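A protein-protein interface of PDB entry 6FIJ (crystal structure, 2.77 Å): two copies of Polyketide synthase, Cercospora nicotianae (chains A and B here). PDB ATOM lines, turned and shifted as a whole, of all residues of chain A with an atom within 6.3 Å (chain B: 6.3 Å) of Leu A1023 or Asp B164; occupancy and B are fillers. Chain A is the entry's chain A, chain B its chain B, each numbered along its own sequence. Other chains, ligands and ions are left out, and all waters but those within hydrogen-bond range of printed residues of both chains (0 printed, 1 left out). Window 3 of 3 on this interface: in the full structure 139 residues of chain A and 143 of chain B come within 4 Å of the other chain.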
ATOM      1  N   TYR A1014       2.672  30.137  13.028  1.00  0.00           N
ATOM      2  CA  TYR A1014       3.454  29.671  14.168  1.00  0.00           C
ATOM      3  C   TYR A1014       2.566  29.455  15.389  1.00  0.00           C
ATOM      4  O   TYR A1014       2.581  28.378  15.998  1.00  0.00           O
ATOM      5  CB  TYR A1014       4.581  30.662  14.464  1.00  0.00           C
ATOM      6  CG  TYR A1014       5.679  30.621  13.423  1.00  0.00           C
ATOM      7  CD1 TYR A1014       6.634  29.614  13.432  1.00  0.00           C
ATOM      8  CD2 TYR A1014       5.755  31.582  12.428  1.00  0.00           C
ATOM      9  CE1 TYR A1014       7.637  29.568  12.482  1.00  0.00           C
ATOM     10  CE2 TYR A1014       6.756  31.546  11.474  1.00  0.00           C
ATOM     11  CZ  TYR A1014       7.695  30.537  11.505  1.00  0.00           C
ATOM     12  OH  TYR A1014       8.693  30.496  10.555  1.00  0.00           O
ATOM     13  N   LEU A1017       0.399  26.519  14.772  1.00  0.00           N
ATOM     14  CA  LEU A1017       1.027  25.212  14.935  1.00  0.00           C
ATOM     15  C   LEU A1017       1.054  24.775  16.393  1.00  0.00           C
ATOM     16  O   LEU A1017       0.988  23.574  16.677  1.00  0.00           O
ATOM     17  CB  LEU A1017       2.449  25.228  14.375  1.00  0.00           C
ATOM     18  CG  LEU A1017       2.627  25.311  12.858  1.00  0.00           C
ATOM     19  CD1 LEU A1017       4.093  25.121  12.514  1.00  0.00           C
ATOM     20  CD2 LEU A1017       1.763  24.295  12.118  1.00  0.00           C
ATOM     21  N   TYR A1018       1.151  25.719  17.330  1.00  0.00           N
ATOM     22  CA  TYR A1018       1.032  25.355  18.737  1.00  0.00           C
ATOM     23  C   TYR A1018      -0.389  24.919  19.062  1.00  0.00           C
ATOM     24  O   TYR A1018      -0.603  23.882  19.699  1.00  0.00           O
ATOM     25  CB  TYR A1018       1.445  26.520  19.635  1.00  0.00           C
ATOM     26  CG  TYR A1018       0.859  26.400  21.021  1.00  0.00           C
ATOM     27  CD1 TYR A1018       1.238  25.368  21.869  1.00  0.00           C
ATOM     28  CD2 TYR A1018      -0.089  27.307  21.476  1.00  0.00           C
ATOM     29  CE1 TYR A1018       0.692  25.245  23.132  1.00  0.00           C
ATOM     30  CE2 TYR A1018      -0.637  27.194  22.739  1.00  0.00           C
ATOM     31  CZ  TYR A1018      -0.241  26.161  23.562  1.00  0.00           C
ATOM     32  OH  TYR A1018      -0.784  26.042  24.819  1.00  0.00           O
ATOM     33  N   ALA A1019      -1.377  25.706  18.631  1.00  0.00           N
ATOM     34  CA  ALA A1019      -2.766  25.347  18.885  1.00  0.00           C
ATOM     35  C   ALA A1019      -3.107  23.988  18.287  1.00  0.00           C
ATOM     36  O   ALA A1019      -3.991  23.290  18.797  1.00  0.00           O
ATOM     37  CB  ALA A1019      -3.691  26.427  18.326  1.00  0.00           C
ATOM     38  N   ALA A1020      -2.414  23.591  17.218  1.00  0.00           N
ATOM     39  CA  ALA A1020      -2.637  22.287  16.609  1.00  0.00           C
ATOM     40  C   ALA A1020      -1.880  21.168  17.313  1.00  0.00           C
ATOM     41  O   ALA A1020      -2.197  19.994  17.094  1.00  0.00           O
ATOM     42  CB  ALA A1020      -2.234  22.321  15.133  1.00  0.00           C
ATOM     43  N   GLY A1021      -0.898  21.498  18.147  1.00  0.00           N
ATOM     44  CA  GLY A1021      -0.129  20.500  18.858  1.00  0.00           C
ATOM     45  C   GLY A1021       1.199  20.131  18.234  1.00  0.00           C
ATOM     46  O   GLY A1021       1.856  19.207  18.726  1.00  0.00           O
ATOM     47  N   VAL A1022       1.620  20.826  17.178  1.00  0.00           N
ATOM     48  CA  VAL A1022       2.849  20.465  16.479  1.00  0.00           C
ATOM     49  C   VAL A1022       4.072  20.906  17.271  1.00  0.00           C
ATOM     50  O   VAL A1022       5.007  20.125  17.486  1.00  0.00           O
ATOM     51  CB  VAL A1022       2.845  21.074  15.063  1.00  0.00           C
ATOM     52  CG1 VAL A1022       4.101  20.677  14.299  1.00  0.00           C
ATOM     53  CG2 VAL A1022       1.600  20.642  14.302  1.00  0.00           C
ATOM     54  N   LEU A1023       4.084  22.159  17.714  1.00  0.00           N
ATOM     55  CA  LEU A1023       5.214  22.747  18.414  1.00  0.00           C
ATOM     56  C   LEU A1023       4.832  23.079  19.849  1.00  0.00           C
ATOM     57  O   LEU A1023       3.668  23.352  20.152  1.00  0.00           O
ATOM     58  CB  LEU A1023       5.691  24.020  17.715  1.00  0.00           C
ATOM     59  CG  LEU A1023       6.303  23.846  16.330  1.00  0.00           C
ATOM     60  CD1 LEU A1023       6.349  25.179  15.611  1.00  0.00           C
ATOM     61  CD2 LEU A1023       7.695  23.255  16.456  1.00  0.00           C
ATOM     62  N   SER A1024       5.828  23.056  20.729  1.00  0.00           N
ATOM     63  CA  SER A1024       5.637  23.550  22.081  1.00  0.00           C
ATOM     64  C   SER A1024       5.730  25.071  22.094  1.00  0.00           C
ATOM     65  O   SER A1024       6.234  25.700  21.160  1.00  0.00           O
ATOM     66  CB  SER A1024       6.676  22.954  23.031  1.00  0.00           C
ATOM     67  OG  SER A1024       7.987  23.344  22.662  1.00  0.00           O
ATOM     68  N   GLN A1025       5.230  25.665  23.178  1.00  0.00           N
ATOM     69  CA  GLN A1025       5.199  27.120  23.271  1.00  0.00           C
ATOM     70  C   GLN A1025       6.602  27.709  23.201  1.00  0.00           C
ATOM     71  O   GLN A1025       6.810  28.759  22.582  1.00  0.00           O
ATOM     72  CB  GLN A1025       4.497  27.541  24.561  1.00  0.00           C
ATOM     73  CG  GLN A1025       3.002  27.288  24.528  1.00  0.00           C
ATOM     74  CD  GLN A1025       2.413  27.060  25.903  1.00  0.00           C
ATOM     75  OE1 GLN A1025       1.972  27.998  26.567  1.00  0.00           O
ATOM     76  NE2 GLN A1025       2.393  25.803  26.334  1.00  0.00           N
ATOM     77  N   SER A1026       7.580  27.045  23.820  1.00  0.00           N
ATOM     78  CA  SER A1026       8.939  27.576  23.821  1.00  0.00           C
ATOM     79  C   SER A1026       9.590  27.428  22.451  1.00  0.00           C
ATOM     80  O   SER A1026      10.301  28.334  21.997  1.00  0.00           O
ATOM     81  CB  SER A1026       9.774  26.883  24.898  1.00  0.00           C
ATOM     82  OG  SER A1026       9.981  25.518  24.587  1.00  0.00           O
ATOM     83  N   ASP A1027       9.369  26.295  21.775  1.00  0.00           N
ATOM     84  CA  ASP A1027       9.910  26.127  20.430  1.00  0.00           C
ATOM     85  C   ASP A1027       9.329  27.160  19.479  1.00  0.00           C
ATOM     86  O   ASP A1027      10.021  27.641  18.574  1.00  0.00           O
ATOM     87  CB  ASP A1027       9.629  24.716  19.910  1.00  0.00           C
ATOM     88  CG  ASP A1027      10.529  23.666  20.533  1.00  0.00           C
ATOM     89  OD1 ASP A1027      11.566  24.032  21.127  1.00  0.00           O
ATOM     90  OD2 ASP A1027      10.202  22.465  20.418  1.00  0.00           O
ATOM     91  N   THR A1028       8.058  27.515  19.665  1.00  0.00           N
ATOM     92  CA  THR A1028       7.462  28.572  18.855  1.00  0.00           C
ATOM     93  C   THR A1028       8.187  29.892  19.079  1.00  0.00           C
ATOM     94  O   THR A1028       8.599  30.560  18.123  1.00  0.00           O
ATOM     95  CB  THR A1028       5.970  28.700  19.180  1.00  0.00           C
ATOM     96  OG1 THR A1028       5.289  27.500  18.790  1.00  0.00           O
ATOM     97  CG2 THR A1028       5.344  29.885  18.451  1.00  0.00           C
ATOM     98  N   LEU A1031      11.614  29.642  17.644  1.00  0.00           N
ATOM     99  CA  LEU A1031      11.588  29.688  16.190  1.00  0.00           C
ATOM    100  C   LEU A1031      11.268  31.091  15.688  1.00  0.00           C
ATOM    101  O   LEU A1031      11.884  31.572  14.730  1.00  0.00           O
ATOM    102  CB  LEU A1031      10.574  28.672  15.667  1.00  0.00           C
ATOM    103  CG  LEU A1031      10.587  28.352  14.173  1.00  0.00           C
ATOM    104  CD1 LEU A1031      11.990  28.050  13.661  1.00  0.00           C
ATOM    105  CD2 LEU A1031       9.667  27.174  13.910  1.00  0.00           C
ATOM    106  N   CYS A1134      13.641  22.175  16.798  1.00  0.00           N
ATOM    107  CA  CYS A1134      12.327  22.003  17.396  1.00  0.00           C
ATOM    108  C   CYS A1134      11.903  20.540  17.371  1.00  0.00           C
ATOM    109  O   CYS A1134      12.303  19.765  16.497  1.00  0.00           O
ATOM    110  CB  CYS A1134      11.295  22.851  16.656  1.00  0.00           C
ATOM    111  SG  CYS A1134      11.702  24.610  16.595  1.00  0.00           S
ATOM    112  N   SER A1135      11.080  20.169  18.349  1.00  0.00           N
ATOM    113  CA  SER A1135      10.536  18.821  18.453  1.00  0.00           C
ATOM    114  C   SER A1135       9.142  18.823  17.840  1.00  0.00           C
ATOM    115  O   SER A1135       8.253  19.539  18.312  1.00  0.00           O
ATOM    116  CB  SER A1135      10.489  18.356  19.908  1.00  0.00           C
ATOM    117  OG  SER A1135      11.791  18.305  20.468  1.00  0.00           O
ATOM    118  N   ILE A1136       8.952  18.013  16.803  1.00  0.00           N
ATOM    119  CA  ILE A1136       7.727  18.010  16.016  1.00  0.00           C
ATOM    120  C   ILE A1136       6.918  16.768  16.356  1.00  0.00           C
ATOM    121  O   ILE A1136       7.469  15.670  16.494  1.00  0.00           O
ATOM    122  CB  ILE A1136       8.040  18.062  14.507  1.00  0.00           C
ATOM    123  CG1 ILE A1136       8.873  19.304  14.167  1.00  0.00           C
ATOM    124  CG2 ILE A1136       6.756  18.035  13.691  1.00  0.00           C
ATOM    125  CD1 ILE A1136       8.181  20.625  14.446  1.00  0.00           C
ATOM    126  N   GLN A1137       5.606  16.947  16.480  1.00  0.00           N
ATOM    127  CA  GLN A1137       4.675  15.851  16.701  1.00  0.00           C
ATOM    128  C   GLN A1137       3.511  15.987  15.732  1.00  0.00           C
ATOM    129  O   GLN A1137       3.261  17.057  15.173  1.00  0.00           O
ATOM    130  CB  GLN A1137       4.136  15.821  18.137  1.00  0.00           C
ATOM    131  CG  GLN A1137       5.118  15.338  19.183  1.00  0.00           C
ATOM    132  CD  GLN A1137       4.425  14.961  20.478  1.00  0.00           C
ATOM    133  OE1 GLN A1137       4.225  13.780  20.767  1.00  0.00           O
ATOM    134  NE2 GLN A1137       4.042  15.965  21.261  1.00  0.00           N
ATOM    135  N   PHE A1163       9.579  25.292   7.286  1.00  0.00           N
ATOM    136  CA  PHE A1163       9.643  26.649   7.815  1.00  0.00           C
ATOM    137  C   PHE A1163      10.415  27.589   6.895  1.00  0.00           C
ATOM    138  O   PHE A1163      10.066  28.769   6.782  1.00  0.00           O
ATOM    139  CB  PHE A1163      10.250  26.620   9.216  1.00  0.00           C
ATOM    140  CG  PHE A1163       9.405  25.881  10.213  1.00  0.00           C
ATOM    141  CD1 PHE A1163       8.297  26.487  10.779  1.00  0.00           C
ATOM    142  CD2 PHE A1163       9.703  24.577  10.565  1.00  0.00           C
ATOM    143  CE1 PHE A1163       7.511  25.812  11.690  1.00  0.00           C
ATOM    144  CE2 PHE A1163       8.919  23.897  11.474  1.00  0.00           C
ATOM    145  CZ  PHE A1163       7.822  24.515  12.037  1.00  0.00           C
ATOM    146  N   GLY B 159       7.386  22.931  32.528  1.00  0.00           N
ATOM    147  CA  GLY B 159       7.509  21.714  31.744  1.00  0.00           C
ATOM    148  C   GLY B 159       6.521  21.666  30.594  1.00  0.00           C
ATOM    149  O   GLY B 159       6.883  21.337  29.461  1.00  0.00           O
ATOM    150  N   SER B 160       5.255  21.990  30.870  1.00  0.00           N
ATOM    151  CA  SER B 160       4.250  21.998  29.811  1.00  0.00           C
ATOM    152  C   SER B 160       4.574  23.045  28.755  1.00  0.00           C
ATOM    153  O   SER B 160       4.399  22.803  27.555  1.00  0.00           O
ATOM    154  CB  SER B 160       2.862  22.254  30.399  1.00  0.00           C
ATOM    155  OG  SER B 160       2.456  21.191  31.241  1.00  0.00           O
ATOM    156  N   CYS B 161       5.043  24.219  29.184  1.00  0.00           N
ATOM    157  CA  CYS B 161       5.420  25.262  28.234  1.00  0.00           C
ATOM    158  C   CYS B 161       6.630  24.853  27.407  1.00  0.00           C
ATOM    159  O   CYS B 161       6.720  25.201  26.225  1.00  0.00           O
ATOM    160  CB  CYS B 161       5.699  26.565  28.980  1.00  0.00           C
ATOM    161  SG  CYS B 161       6.411  27.868  27.957  1.00  0.00           S
ATOM    162  N   LEU B 162       7.561  24.110  28.004  1.00  0.00           N
ATOM    163  CA  LEU B 162       8.751  23.672  27.285  1.00  0.00           C
ATOM    164  C   LEU B 162       8.428  22.528  26.328  1.00  0.00           C
ATOM    165  O   LEU B 162       8.728  22.608  25.132  1.00  0.00           O
ATOM    166  CB  LEU B 162       9.833  23.260  28.284  1.00  0.00           C
ATOM    167  CG  LEU B 162      11.200  22.851  27.733  1.00  0.00           C
ATOM    168  CD1 LEU B 162      11.804  23.950  26.873  1.00  0.00           C
ATOM    169  CD2 LEU B 162      12.130  22.511  28.888  1.00  0.00           C
ATOM    170  N   ALA B 163       7.810  21.461  26.832  1.00  0.00           N
ATOM    171  CA  ALA B 163       7.502  20.288  26.027  1.00  0.00           C
ATOM    172  C   ALA B 163       6.061  19.861  26.264  1.00  0.00           C
ATOM    173  O   ALA B 163       5.590  19.835  27.405  1.00  0.00           O
ATOM    174  CB  ALA B 163       8.445  19.127  26.356  1.00  0.00           C
ATOM    175  N   ASP B 164       5.374  19.514  25.179  1.00  0.00           N
ATOM    176  CA  ASP B 164       4.005  19.032  25.262  1.00  0.00           C
ATOM    177  C   ASP B 164       3.984  17.541  25.572  1.00  0.00           C
ATOM    178  O   ASP B 164       4.908  16.799  25.228  1.00  0.00           O
ATOM    179  CB  ASP B 164       3.260  19.298  23.953  1.00  0.00           C
ATOM    180  CG  ASP B 164       2.902  20.761  23.769  1.00  0.00           C
ATOM    181  OD1 ASP B 164       2.681  21.454  24.786  1.00  0.00           O
ATOM    182  OD2 ASP B 164       2.838  21.217  22.608  1.00  0.00           O
ATOM    183  N   ALA B 165       2.908  17.105  26.221  1.00  0.00           N
ATOM    184  CA  ALA B 165       2.737  15.689  26.506  1.00  0.00           C
ATOM    185  C   ALA B 165       2.635  14.901  25.206  1.00  0.00           C
ATOM    186  O   ALA B 165       2.087  15.373  24.206  1.00  0.00           O
ATOM    187  CB  ALA B 165       1.491  15.465  27.361  1.00  0.00           C
ATOM    188  N   ARG B 166       3.177  13.685  25.223  1.00  0.00           N
ATOM    189  CA  ARG B 166       3.231  12.874  24.019  1.00  0.00           C
ATOM    190  C   ARG B 166       1.846  12.317  23.689  1.00  0.00           C
ATOM    191  O   ARG B 166       0.888  12.446  24.459  1.00  0.00           O
ATOM    192  CB  ARG B 166       4.238  11.734  24.181  1.00  0.00           C
ATOM    193  CG  ARG B 166       5.558  12.139  24.834  1.00  0.00           C
ATOM    194  CD  ARG B 166       6.212  13.332  24.144  1.00  0.00           C
ATOM    195  NE  ARG B 166       6.510  13.077  22.736  1.00  0.00           N
ATOM    196  CZ  ARG B 166       7.133  13.938  21.936  1.00  0.00           C
ATOM    197  NH1 ARG B 166       7.530  15.115  22.401  1.00  0.00           N
ATOM    198  NH2 ARG B 166       7.361  13.621  20.668  1.00  0.00           N
ATOM    199  N   ARG B 167       1.749  11.683  22.517  1.00  0.00           N
ATOM    200  CA  ARG B 167       0.464  11.192  22.034  1.00  0.00           C
ATOM    201  C   ARG B 167       0.079   9.869  22.686  1.00  0.00           C
ATOM    202  O   ARG B 167      -1.104   9.627  22.953  1.00  0.00           O
ATOM    203  CB  ARG B 167       0.504  11.039  20.512  1.00  0.00           C
ATOM    204  CG  ARG B 167       0.668  12.349  19.748  1.00  0.00           C
ATOM    205  CD  ARG B 167      -0.568  13.235  19.865  1.00  0.00           C
ATOM    206  NE  ARG B 167      -0.406  14.510  19.168  1.00  0.00           N
ATOM    207  CZ  ARG B 167       0.083  15.619  19.717  1.00  0.00           C
ATOM    208  NH1 ARG B 167       0.471  15.633  20.988  1.00  0.00           N
ATOM    209  NH2 ARG B 167       0.186  16.723  18.990  1.00  0.00           N
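The backbone carbonyl oxygen (O) of Leu B162 lies within hydrogen-bond range of the side-chain hydroxyl (OG) of Ser A1024 (2.7 Å). The side-chain amide oxygen (OE1) of Gln A1137 is in hydrogen-bond range of the guanidinium group (NE) of Arg B166. N of Gln A1025 lies within hydrogen-bond range of O of Cys B161 (3.4 Å). The backbone carbonyl oxygen (O) of Cys B161 lies within hydrogen-bond range of the backbone NH (N) of Ser A1026, at 3.2 Å. The backbone carbonyl oxygen of Gly A1021 sits at hydrogen-bond distance from the guanidinium group of Arg B167 (3.0 Å). The backbone carbonyl oxygen (O) of Leu A1023 lies close to the side-chain carboxylate (OD2) of Asp B164, 3.4 Å away. OG of Ser A1026 lies within hydrogen-bond range of O of Leu B162 (3.2 Å).
O of Val A1022 is in hydrogen-bond range of N of Gln A1137 (3.4 Å). The backbone carbonyl oxygen of Ser A1024 is in hydrogen-bond range of the side-chain hydroxyl of Thr A1028, 3.1 Å away. The side-chain hydroxyl of Ser A1024 lies within hydrogen-bond range of the side-chain carboxylate of Asp A1027, 3.3 Å away.
Among the printed residues, merely in contact across the chains: Ser A1024 with Cys B161 (3.9 Å), Ser A1024 with Asp B164 (3.7 Å), Gln A1025 with Ser B160 (3.8 Å), Gln A1137 with Ala B165 (3.6 Å) and Gln A1137 with Arg B167 (3.6 Å).
Of the printed residues of chain B, Leu A1023 touches Asp B164. Of chain A, only Leu A1023 and Ser A1024 come within 4 Å of Asp B164. Of the printed residues of chain B, Gln A1025 touches Ser B160 and Cys B161. Printed residues of chain A within 4 Å of Leu B162: Ser A1024 and Ser A1026. Printed residues of chain B within 4 Å of Gly A1021: Arg B167. Ala A1019 touches none of the printed residues of chain B.
Printed residues of chain A that touch a printed residue of chain B: Gly A1021, Leu A1023, Ser A1024, Gln A1025, Ser A1026 and Gln A1137. Along chain A the printed residues that touch a printed residue of chain B span positions 1021 to 1137. Among the printed residues, no Asp or Glu carboxylate lies within 4 Å of a Lys or Arg side-chain nitrogen of the other chain.
No position is printed for both chains.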
